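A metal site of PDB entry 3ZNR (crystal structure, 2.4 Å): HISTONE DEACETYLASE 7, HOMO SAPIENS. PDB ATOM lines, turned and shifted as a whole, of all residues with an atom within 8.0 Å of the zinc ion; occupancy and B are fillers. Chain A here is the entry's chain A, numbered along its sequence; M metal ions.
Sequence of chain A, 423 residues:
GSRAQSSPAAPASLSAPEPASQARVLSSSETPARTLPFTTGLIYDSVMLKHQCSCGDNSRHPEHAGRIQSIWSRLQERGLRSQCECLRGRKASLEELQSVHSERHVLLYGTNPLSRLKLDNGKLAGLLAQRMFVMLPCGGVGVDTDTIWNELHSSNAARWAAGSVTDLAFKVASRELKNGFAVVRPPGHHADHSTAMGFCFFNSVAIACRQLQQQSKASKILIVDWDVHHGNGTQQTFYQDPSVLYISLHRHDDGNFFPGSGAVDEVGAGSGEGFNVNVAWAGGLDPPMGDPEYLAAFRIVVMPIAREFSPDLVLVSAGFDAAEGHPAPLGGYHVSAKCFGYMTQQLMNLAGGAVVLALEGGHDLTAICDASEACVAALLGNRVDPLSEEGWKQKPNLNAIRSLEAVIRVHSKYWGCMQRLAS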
ATOM      1  N   GLN A  52     -13.586  20.159 -24.579  1.00  0.00           N
ATOM      2  CA  GLN A  52     -12.337  19.403 -24.522  1.00  0.00           C
ATOM      3  C   GLN A  52     -12.169  18.559 -25.789  1.00  0.00           C
ATOM      4  O   GLN A  52     -13.151  18.160 -26.414  1.00  0.00           O
ATOM      5  CB  GLN A  52     -12.277  18.522 -23.274  1.00  0.00           C
ATOM      6  CG  GLN A  52     -13.614  17.917 -22.845  1.00  0.00           C
ATOM      7  CD  GLN A  52     -13.505  17.102 -21.567  1.00  0.00           C
ATOM      8  OE1 GLN A  52     -13.964  17.525 -20.501  1.00  0.00           O
ATOM      9  NE2 GLN A  52     -12.881  15.932 -21.668  1.00  0.00           N
ATOM     10  N   CYS A  53     -10.920  18.317 -26.163  1.00  0.00           N
ATOM     11  CA  CYS A  53     -10.594  17.539 -27.354  1.00  0.00           C
ATOM     12  C   CYS A  53     -11.058  16.090 -27.225  1.00  0.00           C
ATOM     13  O   CYS A  53     -11.178  15.567 -26.122  1.00  0.00           O
ATOM     14  CB  CYS A  53      -9.090  17.576 -27.614  1.00  0.00           C
ATOM     15  SG  CYS A  53      -8.586  16.889 -29.205  1.00  0.00           S
ATOM     16  N   SER A  54     -11.313  15.462 -28.372  1.00  0.00           N
ATOM     17  CA  SER A  54     -11.822  14.088 -28.405  1.00  0.00           C
ATOM     18  C   SER A  54     -10.768  13.058 -27.967  1.00  0.00           C
ATOM     19  O   SER A  54     -11.124  11.974 -27.508  1.00  0.00           O
ATOM     20  CB  SER A  54     -12.327  13.745 -29.812  1.00  0.00           C
ATOM     21  OG  SER A  54     -11.320  13.959 -30.781  1.00  0.00           O
ATOM     22  N   CYS A  55      -9.491  13.408 -28.102  1.00  0.00           N
ATOM     23  CA  CYS A  55      -8.398  12.528 -27.678  1.00  0.00           C
ATOM     24  C   CYS A  55      -8.353  12.346 -26.158  1.00  0.00           C
ATOM     25  O   CYS A  55      -7.792  11.364 -25.671  1.00  0.00           O
ATOM     26  CB  CYS A  55      -7.049  13.055 -28.180  1.00  0.00           C
ATOM     27  SG  CYS A  55      -6.525  14.617 -27.442  1.00  0.00           S
ATOM     28  N   GLY A  56      -8.914  13.301 -25.414  1.00  0.00           N
ATOM     29  CA  GLY A  56      -9.094  13.172 -23.973  1.00  0.00           C
ATOM     30  C   GLY A  56      -7.875  13.460 -23.107  1.00  0.00           C
ATOM     31  O   GLY A  56      -7.980  13.446 -21.882  1.00  0.00           O
ATOM     32  N   ASP A  57      -6.729  13.726 -23.736  1.00  0.00           N
ATOM     33  CA  ASP A  57      -5.494  13.978 -23.000  1.00  0.00           C
ATOM     34  C   ASP A  57      -5.433  15.436 -22.534  1.00  0.00           C
ATOM     35  O   ASP A  57      -5.217  16.346 -23.344  1.00  0.00           O
ATOM     36  CB  ASP A  57      -4.279  13.635 -23.873  1.00  0.00           C
ATOM     37  CG  ASP A  57      -3.012  13.399 -23.062  1.00  0.00           C
ATOM     38  OD1 ASP A  57      -2.857  14.006 -21.988  1.00  0.00           O
ATOM     39  OD2 ASP A  57      -2.158  12.609 -23.518  1.00  0.00           O
ATOM     40  N   ASN A  58      -5.639  15.648 -21.240  1.00  0.00           N
ATOM     41  CA  ASN A  58      -5.599  16.995 -20.649  1.00  0.00           C
ATOM     42  C   ASN A  58      -4.186  17.550 -20.490  1.00  0.00           C
ATOM     43  O   ASN A  58      -4.009  18.749 -20.270  1.00  0.00           O
ATOM     44  CB  ASN A  58      -6.325  17.010 -19.294  1.00  0.00           C
ATOM     45  CG  ASN A  58      -7.836  16.950 -19.433  1.00  0.00           C
ATOM     46  OD1 ASN A  58      -8.415  17.467 -20.397  1.00  0.00           O
ATOM     47  ND2 ASN A  58      -8.494  16.345 -18.449  1.00  0.00           N
ATOM     48  N   ARG A  60      -1.722  17.121 -22.972  1.00  0.00           N
ATOM     49  CA  ARG A  60      -1.456  17.670 -24.303  1.00  0.00           C
ATOM     50  C   ARG A  60      -2.290  18.932 -24.589  1.00  0.00           C
ATOM     51  O   ARG A  60      -1.847  19.804 -25.327  1.00  0.00           O
ATOM     52  CB  ARG A  60      -1.712  16.615 -25.390  1.00  0.00           C
ATOM     53  CG  ARG A  60      -1.556  17.137 -26.821  1.00  0.00           C
ATOM     54  CD  ARG A  60      -1.330  16.027 -27.834  1.00  0.00           C
ATOM     55  NE  ARG A  60      -2.325  14.955 -27.713  1.00  0.00           N
ATOM     56  CZ  ARG A  60      -2.055  13.673 -27.417  1.00  0.00           C
ATOM     57  NH1 ARG A  60      -0.818  13.252 -27.206  1.00  0.00           N
ATOM     58  NH2 ARG A  60      -3.059  12.805 -27.347  1.00  0.00           N
ATOM     59  N   HIS A  61      -3.489  18.991 -24.005  1.00  0.00           N
ATOM     60  CA  HIS A  61      -4.360  20.162 -24.132  1.00  0.00           C
ATOM     61  C   HIS A  61      -4.532  20.839 -22.771  1.00  0.00           C
ATOM     62  O   HIS A  61      -5.515  20.580 -22.066  1.00  0.00           O
ATOM     63  CB  HIS A  61      -5.708  19.759 -24.721  1.00  0.00           C
ATOM     64  CG  HIS A  61      -5.596  19.062 -26.047  1.00  0.00           C
ATOM     65  ND1 HIS A  61      -5.093  19.681 -27.169  1.00  0.00           N
ATOM     66  CD2 HIS A  61      -5.920  17.803 -26.420  1.00  0.00           C
ATOM     67  CE1 HIS A  61      -5.109  18.828 -28.183  1.00  0.00           C
ATOM     68  NE2 HIS A  61      -5.606  17.681 -27.748  1.00  0.00           N
ATOM     69  N   LEU A 136      -5.566  17.518 -36.524  1.00  0.00           N
ATOM     70  CA  LEU A 136      -4.488  17.725 -35.564  1.00  0.00           C
ATOM     71  C   LEU A 136      -3.662  16.450 -35.398  1.00  0.00           C
ATOM     72  O   LEU A 136      -4.147  15.363 -35.710  1.00  0.00           O
ATOM     73  CB  LEU A 136      -5.063  18.153 -34.212  1.00  0.00           C
ATOM     74  CG  LEU A 136      -5.934  19.412 -34.204  1.00  0.00           C
ATOM     75  CD1 LEU A 136      -6.538  19.626 -32.832  1.00  0.00           C
ATOM     76  CD2 LEU A 136      -5.130  20.626 -34.644  1.00  0.00           C
ATOM     77  N   PRO A 137      -2.417  16.572 -34.893  1.00  0.00           N
ATOM     78  CA  PRO A 137      -1.548  15.409 -34.673  1.00  0.00           C
ATOM     79  C   PRO A 137      -2.183  14.310 -33.809  1.00  0.00           C
ATOM     80  O   PRO A 137      -2.007  13.131 -34.090  1.00  0.00           O
ATOM     81  CB  PRO A 137      -0.334  16.000 -33.957  1.00  0.00           C
ATOM     82  CG  PRO A 137      -0.291  17.417 -34.382  1.00  0.00           C
ATOM     83  CD  PRO A 137      -1.721  17.831 -34.551  1.00  0.00           C
ATOM     84  N   CYS A 138      -2.919  14.725 -32.778  1.00  0.00           N
ATOM     85  CA  CYS A 138      -3.567  13.785 -31.861  1.00  0.00           C
ATOM     86  C   CYS A 138      -4.804  13.111 -32.461  1.00  0.00           C
ATOM     87  O   CYS A 138      -5.244  12.074 -31.972  1.00  0.00           O
ATOM     88  CB  CYS A 138      -3.958  14.495 -30.565  1.00  0.00           C
ATOM     89  SG  CYS A 138      -5.218  15.764 -30.771  1.00  0.00           S
ATOM     90  N   GLY A 139      -5.371  13.716 -33.506  1.00  0.00           N
ATOM     91  CA  GLY A 139      -6.536  13.152 -34.204  1.00  0.00           C
ATOM     92  C   GLY A 139      -7.768  14.029 -34.170  1.00  0.00           C
ATOM     93  O   GLY A 139      -8.589  13.967 -35.088  1.00  0.00           O
ATOM     94  N   GLY A 140      -7.900  14.852 -33.131  1.00  0.00           N
ATOM     95  CA  GLY A 140      -9.054  15.730 -32.980  1.00  0.00           C
ATOM     96  C   GLY A 140      -9.077  16.876 -33.964  1.00  0.00           C
ATOM     97  O   GLY A 140      -8.131  17.062 -34.733  1.00  0.00           O
ATOM     98  N   VAL A 141     -10.164  17.639 -33.944  1.00  0.00           N
ATOM     99  CA  VAL A 141     -10.332  18.793 -34.826  1.00  0.00           C
ATOM    100  C   VAL A 141     -10.093  20.079 -34.049  1.00  0.00           C
ATOM    101  O   VAL A 141     -10.350  20.142 -32.846  1.00  0.00           O
ATOM    102  CB  VAL A 141     -11.747  18.800 -35.462  1.00  0.00           C
ATOM    103  CG1 VAL A 141     -12.014  20.122 -36.170  1.00  0.00           C
ATOM    104  CG2 VAL A 141     -11.886  17.641 -36.423  1.00  0.00           C
ATOM    105  N   THR A 145      -3.160  23.995 -33.714  1.00  0.00           N
ATOM    106  CA  THR A 145      -2.606  22.953 -32.841  1.00  0.00           C
ATOM    107  C   THR A 145      -2.950  23.145 -31.355  1.00  0.00           C
ATOM    108  O   THR A 145      -3.131  22.173 -30.634  1.00  0.00           O
ATOM    109  CB  THR A 145      -1.071  22.847 -32.975  1.00  0.00           C
ATOM    110  OG1 THR A 145      -0.482  24.138 -32.757  1.00  0.00           O
ATOM    111  CG2 THR A 145      -0.689  22.351 -34.365  1.00  0.00           C
ATOM    112  N   ILE A 148      -8.259  23.812 -29.786  1.00  0.00           N
ATOM    113  CA  ILE A 148      -9.023  22.636 -30.191  1.00  0.00           C
ATOM    114  C   ILE A 148     -10.498  22.968 -30.406  1.00  0.00           C
ATOM    115  O   ILE A 148     -10.953  24.050 -30.039  1.00  0.00           O
ATOM    116  CB  ILE A 148      -8.879  21.471 -29.155  1.00  0.00           C
ATOM    117  CG1 ILE A 148      -9.582  21.788 -27.830  1.00  0.00           C
ATOM    118  CG2 ILE A 148      -7.407  21.154 -28.925  1.00  0.00           C
ATOM    119  CD1 ILE A 148     -11.019  21.326 -27.771  1.00  0.00           C
ATOM    120  N   TRP A 149     -11.235  22.034 -31.010  1.00  0.00           N
ATOM    121  CA  TRP A 149     -12.651  22.231 -31.295  1.00  0.00           C
ATOM    122  C   TRP A 149     -13.453  20.944 -31.167  1.00  0.00           C
ATOM    123  O   TRP A 149     -13.368  20.052 -32.021  1.00  0.00           O
ATOM    124  CB  TRP A 149     -12.842  22.816 -32.693  1.00  0.00           C
ATOM    125  CG  TRP A 149     -14.267  23.134 -33.026  1.00  0.00           C
ATOM    126  CD1 TRP A 149     -15.099  22.412 -33.834  1.00  0.00           C
ATOM    127  CD2 TRP A 149     -15.035  24.245 -32.554  1.00  0.00           C
ATOM    128  NE1 TRP A 149     -16.341  23.004 -33.890  1.00  0.00           N
ATOM    129  CE2 TRP A 149     -16.330  24.137 -33.110  1.00  0.00           C
ATOM    130  CE3 TRP A 149     -14.758  25.318 -31.698  1.00  0.00           C
ATOM    131  CZ2 TRP A 149     -17.334  25.066 -32.852  1.00  0.00           C
ATOM    132  CZ3 TRP A 149     -15.762  26.246 -31.440  1.00  0.00           C
ATOM    133  CH2 TRP A 149     -17.033  26.114 -32.023  1.00  0.00           C
HETATM  134 ZN    ZN M   1      -6.363  16.145 -28.830  1.00  0.00          ZN
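The side-chain sulfur of Cys 138 sits close to the backbone NH of Gly 140.
Of the 18 residues printed, 4 come within 4 Å of the zinc ion.
The zinc ion is bound by NE2 of His 61 (2.0 Å), SG of Cys 55 (2.1 Å), SG of Cys 138 (2.3 Å) and SG of Cys 53 (2.4 Å).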
